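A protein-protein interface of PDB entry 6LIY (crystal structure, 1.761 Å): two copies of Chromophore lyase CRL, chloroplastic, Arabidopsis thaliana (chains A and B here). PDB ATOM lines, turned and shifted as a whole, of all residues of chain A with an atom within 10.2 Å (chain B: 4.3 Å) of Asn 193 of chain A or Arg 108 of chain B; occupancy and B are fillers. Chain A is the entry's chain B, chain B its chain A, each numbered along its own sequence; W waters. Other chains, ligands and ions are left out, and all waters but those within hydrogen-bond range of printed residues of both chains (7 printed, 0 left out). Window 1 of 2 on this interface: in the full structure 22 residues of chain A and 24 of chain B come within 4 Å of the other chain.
The backbone carbonyl oxygen (O) of Pro 106 of chain B sits at hydrogen-bond distance from the side-chain amino group (NZ) of Lys 228 of chain A, at 3.4 Å. The side-chain amide nitrogen (ND2) of Asn 193 of chain A sits close to the guanidinium group (NH2) of Arg 108 of chain B (3.2 Å). The guanidinium group (NH2) of Arg 110 of chain B lies within hydrogen-bond range of the side-chain amide oxygen (OD1) of Asn 193 of chain A (3.0 Å).
O of Leu 95 of chain B lies within hydrogen-bond range of N of Arg 110 of chain B. The backbone NH of Phe 107 of chain B lies within hydrogen-bond range of the backbone carbonyl oxygen of Gln 97 of chain B, 2.9 Å away. The backbone NH (N) of Gln 97 of chain B is in hydrogen-bond range of the backbone carbonyl oxygen (O) of Arg 108 of chain B, 3.0 Å away. The side-chain amide oxygen (OD1) of Asn 190 of chain A sits at hydrogen-bond distance from the backbone NH (N) of Trp 192 of chain A (3.0 Å). The backbone NH (N) of Val 224 of chain A lies within hydrogen-bond range of the backbone carbonyl oxygen (O) of Gly 216 of chain A (2.7 Å).
Among the printed residues, pairs that only touch across the chains: Trp 192 of chain A with Trp 225 of chain B (3.8 Å), Asn 193 of chain A with Trp 225 of chain B (3.2 Å) and Val 224 of chain A with Phe 107 of chain B (3.9 Å).
Arg 108 of chain A touches none of the printed residues of chain B. Of chain B, only Arg 108 (3.2 Å), Arg 110 (3.0 Å) and Trp 225 (3.2 Å) come within 4 Å of Asn 193 of chain A. Ser 196 of chain A touches none of the printed residues of chain B. Of the printed residues of chain B, Val 224 of chain A touches Phe 107. No residue of chain A comes within 4 Å of Gln 97 of chain B. Printed residues of chain A within 4 Å of Pro 106 of chain B: Lys 228. Phe 107 of chain B touches one residue of chain A. Arg 108 of chain B touches just one residue of chain A: Asn 193 (3.2 Å). Printed residues of chain A within 4 Å of Arg 110 of chain B: Asn 193 (3.0 Å). Printed residues of chain A within 4 Å of Trp 225 of chain B: Trp 192 and Asn 193. The nearest residue of chain A that does not touch Arg 108 of chain B is Val 224 of chain A (5.5 Å).
Hydrophobic or aromatic side chains of chain A that line the printed part of chain B: Trp 192. Printed residues of chain B that touch a printed residue of chain A: Pro 106, Phe 107, Arg 108, Arg 110 and Trp 225.
2 positions are printed for both chains. Of the 6 pairs that touch across the chains among the printed residues, none has its exchanged pair printed and touching as well.
Water W4 bridges O of Pro 106 of chain B (2.7 Å) and NZ of Lys 228 of chain A (2.7 Å). Water W7 bridges the backbone carbonyl oxygen (O) of Asn 193 of chain A (2.7 Å) and the guanidinium group (NH1) of Arg 110 of chain B (2.9 Å). Water W1 lies within hydrogen-bond range of the backbone carbonyl oxygen (O) of Val 224 of chain A (2.8 Å), the backbone carbonyl oxygen (O) of Phe 107 of chain B (3.0 Å) and the guanidinium group (NE) of Arg 108 of chain B (3.2 Å). Water W5 lies within hydrogen-bond range of the side-chain amide oxygen (OD1) of Asn 193 of chain A (2.9 Å) and the guanidinium group (NE) of Arg 110 of chain B (3.1 Å). Water W6 bridges the backbone carbonyl oxygen of Phe 107 of chain B (3.0 Å) and the backbone carbonyl oxygen of Val 224 of chain A (3.5 Å). Water W3 lies within hydrogen-bond range of OE1 of Gln 109 of chain B and O of Gln 223 of chain A.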
ATOM      1  N   ARG A 108      32.225  10.888   1.875  1.00  0.00           N
ATOM      2  CA  ARG A 108      31.779  10.909   3.259  1.00  0.00           C
ATOM      3  C   ARG A 108      32.960  11.293   4.139  1.00  0.00           C
ATOM      4  O   ARG A 108      34.062  10.780   3.955  1.00  0.00           O
ATOM      5  CB  ARG A 108      31.199   9.551   3.659  1.00  0.00           C
ATOM      6  CG  ARG A 108      30.550   9.527   5.043  1.00  0.00           C
ATOM      7  CD  ARG A 108      29.614   8.355   5.179  1.00  0.00           C
ATOM      8  NE  ARG A 108      28.669   8.317   4.068  1.00  0.00           N
ATOM      9  CZ  ARG A 108      28.027   7.221   3.687  1.00  0.00           C
ATOM     10  NH1 ARG A 108      28.221   6.090   4.351  1.00  0.00           N
ATOM     11  NH2 ARG A 108      27.185   7.256   2.656  1.00  0.00           N
ATOM     12  N   ASN A 190      17.765   9.988  10.609  1.00  0.00           N
ATOM     13  CA  ASN A 190      18.454  10.357   9.381  1.00  0.00           C
ATOM     14  C   ASN A 190      17.400  10.709   8.347  1.00  0.00           C
ATOM     15  O   ASN A 190      16.346  10.073   8.303  1.00  0.00           O
ATOM     16  CB  ASN A 190      19.341   9.211   8.887  1.00  0.00           C
ATOM     17  CG  ASN A 190      19.954   9.503   7.528  1.00  0.00           C
ATOM     18  OD1 ASN A 190      19.376   9.177   6.488  1.00  0.00           O
ATOM     19  ND2 ASN A 190      21.110  10.146   7.534  1.00  0.00           N
ATOM     20  N   SER A 191      17.684  11.712   7.502  1.00  0.00           N
ATOM     21  CA  SER A 191      16.683  12.179   6.543  1.00  0.00           C
ATOM     22  C   SER A 191      17.190  12.178   5.100  1.00  0.00           C
ATOM     23  O   SER A 191      16.669  12.922   4.265  1.00  0.00           O
ATOM     24  CB  SER A 191      16.174  13.575   6.913  1.00  0.00           C
ATOM     25  OG  SER A 191      17.232  14.516   7.003  1.00  0.00           O
ATOM     26  N   TRP A 192      18.175  11.343   4.771  1.00  0.00           N
ATOM     27  CA  TRP A 192      18.681  11.276   3.400  1.00  0.00           C
ATOM     28  C   TRP A 192      17.731  10.487   2.509  1.00  0.00           C
ATOM     29  O   TRP A 192      17.491   9.298   2.753  1.00  0.00           O
ATOM     30  CB  TRP A 192      20.048  10.599   3.350  1.00  0.00           C
ATOM     31  CG  TRP A 192      21.144  11.276   4.066  1.00  0.00           C
ATOM     32  CD1 TRP A 192      21.080  12.424   4.791  1.00  0.00           C
ATOM     33  CD2 TRP A 192      22.498  10.828   4.130  1.00  0.00           C
ATOM     34  NE1 TRP A 192      22.320  12.731   5.300  1.00  0.00           N
ATOM     35  CE2 TRP A 192      23.208  11.760   4.913  1.00  0.00           C
ATOM     36  CE3 TRP A 192      23.180   9.729   3.598  1.00  0.00           C
ATOM     37  CZ2 TRP A 192      24.568  11.628   5.181  1.00  0.00           C
ATOM     38  CZ3 TRP A 192      24.545   9.595   3.876  1.00  0.00           C
ATOM     39  CH2 TRP A 192      25.217  10.546   4.652  1.00  0.00           C
ATOM     40  N   ASN A 193      17.251  11.120   1.435  1.00  0.00           N
ATOM     41  CA  ASN A 193      16.563  10.404   0.363  1.00  0.00           C
ATOM     42  C   ASN A 193      15.302   9.709   0.865  1.00  0.00           C
ATOM     43  O   ASN A 193      14.992   8.586   0.464  1.00  0.00           O
ATOM     44  CB  ASN A 193      17.497   9.399  -0.313  1.00  0.00           C
ATOM     45  CG  ASN A 193      17.921   9.843  -1.702  1.00  0.00           C
ATOM     46  OD1 ASN A 193      17.147  10.460  -2.437  1.00  0.00           O
ATOM     47  ND2 ASN A 193      19.158   9.540  -2.061  1.00  0.00           N
ATOM     48  N   GLY A 194      14.559  10.390   1.735  1.00  0.00           N
ATOM     49  CA  GLY A 194      13.346   9.818   2.274  1.00  0.00           C
ATOM     50  C   GLY A 194      13.556   8.853   3.416  1.00  0.00           C
ATOM     51  O   GLY A 194      12.602   8.184   3.831  1.00  0.00           O
ATOM     52  N   ALA A 195      14.776   8.741   3.926  1.00  0.00           N
ATOM     53  CA  ALA A 195      14.984   7.946   5.128  1.00  0.00           C
ATOM     54  C   ALA A 195      14.353   8.633   6.340  1.00  0.00           C
ATOM     55  O   ALA A 195      14.106   9.842   6.343  1.00  0.00           O
ATOM     56  CB  ALA A 195      16.479   7.727   5.372  1.00  0.00           C
ATOM     57  N   SER A 196      14.094   7.841   7.394  1.00  0.00           N
ATOM     58  CA  SER A 196      13.824   8.409   8.711  1.00  0.00           C
ATOM     59  C   SER A 196      14.824   7.983   9.781  1.00  0.00           C
ATOM     60  O   SER A 196      14.909   8.638  10.825  1.00  0.00           O
ATOM     61  CB  SER A 196      12.408   8.053   9.194  1.00  0.00           C
ATOM     62  OG  SER A 196      12.240   6.659   9.371  1.00  0.00           O
ATOM     63  N   TYR A 197      15.591   6.930   9.549  1.00  0.00           N
ATOM     64  CA  TYR A 197      16.606   6.546  10.511  1.00  0.00           C
ATOM     65  C   TYR A 197      17.737   5.853   9.776  1.00  0.00           C
ATOM     66  O   TYR A 197      17.608   5.443   8.624  1.00  0.00           O
ATOM     67  CB  TYR A 197      16.029   5.641  11.608  1.00  0.00           C
ATOM     68  CG  TYR A 197      15.565   4.265  11.142  1.00  0.00           C
ATOM     69  CD1 TYR A 197      14.296   4.072  10.602  1.00  0.00           C
ATOM     70  CD2 TYR A 197      16.372   3.148  11.303  1.00  0.00           C
ATOM     71  CE1 TYR A 197      13.870   2.805  10.205  1.00  0.00           C
ATOM     72  CE2 TYR A 197      15.945   1.886  10.910  1.00  0.00           C
ATOM     73  CZ  TYR A 197      14.695   1.726  10.367  1.00  0.00           C
ATOM     74  OH  TYR A 197      14.278   0.474   9.967  1.00  0.00           O
ATOM     75  N   ARG A 215      23.687   2.209   6.848  1.00  0.00           N
ATOM     76  CA  ARG A 215      22.475   2.082   6.038  1.00  0.00           C
ATOM     77  C   ARG A 215      21.432   3.076   6.508  1.00  0.00           C
ATOM     78  O   ARG A 215      21.308   3.306   7.705  1.00  0.00           O
ATOM     79  CB  ARG A 215      21.835   0.702   6.175  1.00  0.00           C
ATOM     80  CG  ARG A 215      22.675  -0.470   5.790  1.00  0.00           C
ATOM     81  CD  ARG A 215      21.809  -1.715   5.829  1.00  0.00           C
ATOM     82  NE  ARG A 215      21.879  -2.381   7.126  1.00  0.00           N
ATOM     83  CZ  ARG A 215      21.262  -3.525   7.413  1.00  0.00           C
ATOM     84  NH1 ARG A 215      20.516  -4.125   6.500  1.00  0.00           N
ATOM     85  NH2 ARG A 215      21.388  -4.061   8.619  1.00  0.00           N
ATOM     86  N   GLY A 216      20.619   3.589   5.586  1.00  0.00           N
ATOM     87  CA  GLY A 216      19.479   4.414   5.944  1.00  0.00           C
ATOM     88  C   GLY A 216      18.186   3.736   5.529  1.00  0.00           C
ATOM     89  O   GLY A 216      18.131   3.039   4.517  1.00  0.00           O
ATOM     90  N   PHE A 217      17.138   3.945   6.331  1.00  0.00           N
ATOM     91  CA  PHE A 217      15.849   3.308   6.121  1.00  0.00           C
ATOM     92  C   PHE A 217      14.743   4.345   6.221  1.00  0.00           C
ATOM     93  O   PHE A 217      14.865   5.335   6.951  1.00  0.00           O
ATOM     94  CB  PHE A 217      15.562   2.204   7.153  1.00  0.00           C
ATOM     95  CG  PHE A 217      16.508   1.048   7.102  1.00  0.00           C
ATOM     96  CD1 PHE A 217      17.676   1.057   7.853  1.00  0.00           C
ATOM     97  CD2 PHE A 217      16.210  -0.069   6.342  1.00  0.00           C
ATOM     98  CE1 PHE A 217      18.546  -0.011   7.817  1.00  0.00           C
ATOM     99  CE2 PHE A 217      17.069  -1.147   6.301  1.00  0.00           C
ATOM    100  CZ  PHE A 217      18.247  -1.122   7.042  1.00  0.00           C
ATOM    101  N   ASP A 218      13.650   4.100   5.503  1.00  0.00           N
ATOM    102  CA  ASP A 218      12.525   5.012   5.603  1.00  0.00           C
ATOM    103  C   ASP A 218      11.595   4.592   6.735  1.00  0.00           C
ATOM    104  O   ASP A 218      11.754   3.533   7.348  1.00  0.00           O
ATOM    105  CB  ASP A 218      11.762   5.113   4.275  1.00  0.00           C
ATOM    106  CG  ASP A 218      11.172   3.786   3.801  1.00  0.00           C
ATOM    107  OD1 ASP A 218      11.005   2.835   4.599  1.00  0.00           O
ATOM    108  OD2 ASP A 218      10.870   3.696   2.587  1.00  0.00           O
ATOM    109  N   GLU A 219      10.590   5.441   6.978  1.00  0.00           N
ATOM    110  CA  GLU A 219       9.652   5.243   8.078  1.00  0.00           C
ATOM    111  C   GLU A 219       9.027   3.858   8.071  1.00  0.00           C
ATOM    112  O   GLU A 219       8.586   3.388   9.125  1.00  0.00           O
ATOM    113  CB  GLU A 219       8.543   6.301   8.019  1.00  0.00           C
ATOM    114  CG  GLU A 219       8.995   7.709   8.379  1.00  0.00           C
ATOM    115  CD  GLU A 219       7.888   8.564   8.978  1.00  0.00           C
ATOM    116  OE1 GLU A 219       8.196   9.689   9.428  1.00  0.00           O
ATOM    117  OE2 GLU A 219       6.719   8.115   9.002  1.00  0.00           O
ATOM    118  N   ASN A 222      12.113   0.310   4.728  1.00  0.00           N
ATOM    119  CA  ASN A 222      12.760   0.004   3.457  1.00  0.00           C
ATOM    120  C   ASN A 222      14.117   0.692   3.395  1.00  0.00           C
ATOM    121  O   ASN A 222      14.247   1.862   3.762  1.00  0.00           O
ATOM    122  CB  ASN A 222      11.913   0.471   2.265  1.00  0.00           C
ATOM    123  CG  ASN A 222      10.500  -0.057   2.305  1.00  0.00           C
ATOM    124  OD1 ASN A 222       9.608   0.570   2.868  1.00  0.00           O
ATOM    125  ND2 ASN A 222      10.284  -1.203   1.686  1.00  0.00           N
ATOM    126  N   GLN A 223      15.128  -0.025   2.916  1.00  0.00           N
ATOM    127  CA  GLN A 223      16.440   0.593   2.829  1.00  0.00           C
ATOM    128  C   GLN A 223      16.463   1.634   1.719  1.00  0.00           C
ATOM    129  O   GLN A 223      15.906   1.431   0.636  1.00  0.00           O
ATOM    130  CB  GLN A 223      17.531  -0.443   2.597  1.00  0.00           C
ATOM    131  CG  GLN A 223      18.923   0.165   2.633  1.00  0.00           C
ATOM    132  CD  GLN A 223      20.011  -0.878   2.698  1.00  0.00           C
ATOM    133  OE1 GLN A 223      19.734  -2.072   2.843  1.00  0.00           O
ATOM    134  NE2 GLN A 223      21.265  -0.434   2.606  1.00  0.00           N
ATOM    135  N   VAL A 224      17.104   2.758   2.010  1.00  0.00           N
ATOM    136  CA  VAL A 224      17.101   3.914   1.121  1.00  0.00           C
ATOM    137  C   VAL A 224      18.509   4.370   0.733  1.00  0.00           C
ATOM    138  O   VAL A 224      18.669   5.033  -0.306  1.00  0.00           O
ATOM    139  CB  VAL A 224      16.302   5.063   1.774  1.00  0.00           C
ATOM    140  CG1 VAL A 224      16.766   6.428   1.326  1.00  0.00           C
ATOM    141  CG2 VAL A 224      14.805   4.870   1.508  1.00  0.00           C
ATOM    142  N   TRP A 225      19.544   4.044   1.505  1.00  0.00           N
ATOM    143  CA  TRP A 225      20.923   4.282   1.097  1.00  0.00           C
ATOM    144  C   TRP A 225      21.827   3.277   1.803  1.00  0.00           C
ATOM    145  O   TRP A 225      21.421   2.611   2.760  1.00  0.00           O
ATOM    146  CB  TRP A 225      21.385   5.729   1.363  1.00  0.00           C
ATOM    147  CG  TRP A 225      21.301   6.253   2.786  1.00  0.00           C
ATOM    148  CD1 TRP A 225      20.294   7.017   3.320  1.00  0.00           C
ATOM    149  CD2 TRP A 225      22.276   6.090   3.833  1.00  0.00           C
ATOM    150  NE1 TRP A 225      20.582   7.331   4.626  1.00  0.00           N
ATOM    151  CE2 TRP A 225      21.788   6.774   4.970  1.00  0.00           C
ATOM    152  CE3 TRP A 225      23.516   5.441   3.914  1.00  0.00           C
ATOM    153  CZ2 TRP A 225      22.484   6.809   6.192  1.00  0.00           C
ATOM    154  CZ3 TRP A 225      24.213   5.476   5.136  1.00  0.00           C
ATOM    155  CH2 TRP A 225      23.691   6.168   6.248  1.00  0.00           C
ATOM    156  N   GLY A 226      23.051   3.136   1.284  1.00  0.00           N
ATOM    157  CA  GLY A 226      24.014   2.211   1.834  1.00  0.00           C
ATOM    158  C   GLY A 226      23.996   0.866   1.124  1.00  0.00           C
ATOM    159  O   GLY A 226      23.046   0.539   0.407  1.00  0.00           O
ATOM    160  N   LYS A 228      23.371  -2.952   0.247  1.00  0.00           N
ATOM    161  CA  LYS A 228      22.199  -3.746   0.591  1.00  0.00           C
ATOM    162  C   LYS A 228      22.529  -5.136   1.120  1.00  0.00           C
ATOM    163  O   LYS A 228      21.757  -5.679   1.916  1.00  0.00           O
ATOM    164  CB  LYS A 228      21.279  -3.870  -0.626  1.00  0.00           C
ATOM    165  CG  LYS A 228      20.192  -2.816  -0.661  1.00  0.00           C
ATOM    166  CD  LYS A 228      18.866  -3.351  -0.098  1.00  0.00           C
ATOM    167  CE  LYS A 228      17.677  -2.507  -0.583  1.00  0.00           C
ATOM    168  NZ  LYS A 228      17.715  -2.261  -2.064  1.00  0.00           N
ATOM    169  N   LEU B  95       9.115   5.418 -11.191  1.00  0.00           N
ATOM    170  CA  LEU B  95      10.469   5.375 -11.741  1.00  0.00           C
ATOM    171  C   LEU B  95      11.409   4.746 -10.723  1.00  0.00           C
ATOM    172  O   LEU B  95      11.385   5.107  -9.539  1.00  0.00           O
ATOM    173  CB  LEU B  95      10.944   6.781 -12.092  1.00  0.00           C
ATOM    174  CG  LEU B  95      12.188   6.936 -12.966  1.00  0.00           C
ATOM    175  CD1 LEU B  95      12.052   8.225 -13.755  1.00  0.00           C
ATOM    176  CD2 LEU B  95      13.464   6.935 -12.092  1.00  0.00           C
ATOM    177  N   GLU B  96      12.237   3.815 -11.172  1.00  0.00           N
ATOM    178  CA  GLU B  96      13.247   3.241 -10.298  1.00  0.00           C
ATOM    179  C   GLU B  96      14.594   3.236 -11.002  1.00  0.00           C
ATOM    180  O   GLU B  96      14.681   3.230 -12.235  1.00  0.00           O
ATOM    181  CB  GLU B  96      12.875   1.822  -9.813  1.00  0.00           C
ATOM    182  CG  GLU B  96      12.796   0.720 -10.876  1.00  0.00           C
ATOM    183  CD  GLU B  96      12.256  -0.616 -10.317  1.00  0.00           C
ATOM    184  OE1 GLU B  96      11.543  -0.619  -9.284  1.00  0.00           O
ATOM    185  OE2 GLU B  96      12.539  -1.666 -10.923  1.00  0.00           O
ATOM    186  N   GLN B  97      15.647   3.265 -10.185  1.00  0.00           N
ATOM    187  CA  GLN B  97      17.020   3.241 -10.659  1.00  0.00           C
ATOM    188  C   GLN B  97      17.723   2.087  -9.986  1.00  0.00           C
ATOM    189  O   GLN B  97      17.488   1.826  -8.802  1.00  0.00           O
ATOM    190  CB  GLN B  97      17.760   4.539 -10.332  1.00  0.00           C
ATOM    191  CG  GLN B  97      17.256   5.759 -11.022  1.00  0.00           C
ATOM    192  CD  GLN B  97      18.105   6.965 -10.704  1.00  0.00           C
ATOM    193  OE1 GLN B  97      19.328   6.922 -10.817  1.00  0.00           O
ATOM    194  NE2 GLN B  97      17.464   8.045 -10.288  1.00  0.00           N
ATOM    195  N   PRO B 106      16.558  -2.270  -7.102  1.00  0.00           N
ATOM    196  CA  PRO B 106      16.698  -0.818  -7.260  1.00  0.00           C
ATOM    197  C   PRO B 106      17.190  -0.178  -5.974  1.00  0.00           C
ATOM    198  O   PRO B 106      16.809  -0.585  -4.872  1.00  0.00           O
ATOM    199  CB  PRO B 106      15.279  -0.359  -7.604  1.00  0.00           C
ATOM    200  CG  PRO B 106      14.394  -1.432  -7.055  1.00  0.00           C
ATOM    201  CD  PRO B 106      15.163  -2.703  -7.274  1.00  0.00           C
ATOM    202  N   PHE B 107      18.062   0.820  -6.121  1.00  0.00           N
ATOM    203  CA  PHE B 107      18.491   1.614  -4.975  1.00  0.00           C
ATOM    204  C   PHE B 107      17.656   2.871  -4.791  1.00  0.00           C
ATOM    205  O   PHE B 107      17.757   3.508  -3.738  1.00  0.00           O
ATOM    206  CB  PHE B 107      19.974   2.000  -5.091  1.00  0.00           C
ATOM    207  CG  PHE B 107      20.294   2.870  -6.292  1.00  0.00           C
ATOM    208  CD1 PHE B 107      20.181   4.254  -6.217  1.00  0.00           C
ATOM    209  CD2 PHE B 107      20.739   2.301  -7.476  1.00  0.00           C
ATOM    210  CE1 PHE B 107      20.466   5.053  -7.297  1.00  0.00           C
ATOM    211  CE2 PHE B 107      21.044   3.101  -8.576  1.00  0.00           C
ATOM    212  CZ  PHE B 107      20.904   4.473  -8.493  1.00  0.00           C
ATOM    213  N   ARG B 108      16.846   3.251  -5.783  1.00  0.00           N
ATOM    214  CA  ARG B 108      15.972   4.406  -5.661  1.00  0.00           C
ATOM    215  C   ARG B 108      14.625   4.124  -6.311  1.00  0.00           C
ATOM    216  O   ARG B 108      14.568   3.613  -7.429  1.00  0.00           O
ATOM    217  CB  ARG B 108      16.581   5.653  -6.310  1.00  0.00           C
ATOM    218  CG  ARG B 108      15.876   6.905  -5.862  1.00  0.00           C
ATOM    219  CD  ARG B 108      16.806   8.066  -5.812  1.00  0.00           C
ATOM    220  NE  ARG B 108      18.007   7.770  -5.041  1.00  0.00           N
ATOM    221  CZ  ARG B 108      19.185   8.309  -5.320  1.00  0.00           C
ATOM    222  NH1 ARG B 108      19.285   9.137  -6.350  1.00  0.00           N
ATOM    223  NH2 ARG B 108      20.251   8.009  -4.593  1.00  0.00           N
ATOM    224  N   GLN B 109      13.547   4.500  -5.625  1.00  0.00           N
ATOM    225  CA  GLN B 109      12.200   4.305  -6.148  1.00  0.00           C
ATOM    226  C   GLN B 109      11.405   5.572  -5.907  1.00  0.00           C
ATOM    227  O   GLN B 109      11.352   6.057  -4.771  1.00  0.00           O
ATOM    228  CB  GLN B 109      11.516   3.106  -5.476  1.00  0.00           C
ATOM    229  CG  GLN B 109      12.111   1.765  -5.838  1.00  0.00           C
ATOM    230  CD  GLN B 109      11.553   0.654  -4.980  1.00  0.00           C
ATOM    231  OE1 GLN B 109      12.106   0.339  -3.915  1.00  0.00           O
ATOM    232  NE2 GLN B 109      10.460   0.049  -5.427  1.00  0.00           N
ATOM    233  N   ARG B 110      10.798   6.121  -6.967  1.00  0.00           N
ATOM    234  CA  ARG B 110      10.087   7.376  -6.864  1.00  0.00           C
ATOM    235  C   ARG B 110       8.763   7.292  -7.609  1.00  0.00           C
ATOM    236  O   ARG B 110       8.556   6.436  -8.471  1.00  0.00           O
ATOM    237  CB  ARG B 110      10.914   8.550  -7.415  1.00  0.00           C
ATOM    238  CG  ARG B 110      12.242   8.750  -6.680  1.00  0.00           C
ATOM    239  CD  ARG B 110      12.061   9.621  -5.450  1.00  0.00           C
ATOM    240  NE  ARG B 110      13.266   9.677  -4.622  1.00  0.00           N
ATOM    241  CZ  ARG B 110      13.504   8.857  -3.600  1.00  0.00           C
ATOM    242  NH1 ARG B 110      12.618   7.929  -3.260  1.00  0.00           N
ATOM    243  NH2 ARG B 110      14.613   8.985  -2.889  1.00  0.00           N
ATOM    244  N   TRP B 225      24.959  13.091  -0.560  1.00  0.00           N
ATOM    245  CA  TRP B 225      24.729  12.009  -1.506  1.00  0.00           C
ATOM    246  C   TRP B 225      24.513  12.589  -2.898  1.00  0.00           C
ATOM    247  O   TRP B 225      24.349  13.803  -3.081  1.00  0.00           O
ATOM    248  CB  TRP B 225      23.555  11.101  -1.077  1.00  0.00           C
ATOM    249  CG  TRP B 225      22.226  11.787  -0.881  1.00  0.00           C
ATOM    250  CD1 TRP B 225      21.693  12.214   0.298  1.00  0.00           C
ATOM    251  CD2 TRP B 225      21.246  12.079  -1.890  1.00  0.00           C
ATOM    252  NE1 TRP B 225      20.457  12.772   0.088  1.00  0.00           N
ATOM    253  CE2 TRP B 225      20.156  12.693  -1.246  1.00  0.00           C
ATOM    254  CE3 TRP B 225      21.190  11.885  -3.275  1.00  0.00           C
ATOM    255  CZ2 TRP B 225      19.027  13.127  -1.938  1.00  0.00           C
ATOM    256  CZ3 TRP B 225      20.061  12.314  -3.961  1.00  0.00           C
ATOM    257  CH2 TRP B 225      18.999  12.922  -3.292  1.00  0.00           C
HETATM  258  O   HOH W   1      17.155   6.135  -2.393  1.00  0.00           O
HETATM  259  O   HOH W   2      20.611   5.638  -2.483  1.00  0.00           O
HETATM  260  O   HOH W   3      14.149   2.239  -2.096  1.00  0.00           O
HETATM  261  O   HOH W   4      15.697  -2.824  -3.842  1.00  0.00           O
HETATM  262  O   HOH W   5      15.935  11.277  -4.995  1.00  0.00           O
HETATM  263  O   HOH W   6      18.680   1.765  -1.477  1.00  0.00           O
HETATM  264  O   HOH W   7      13.040   7.014  -0.577  1.00  0.00           O
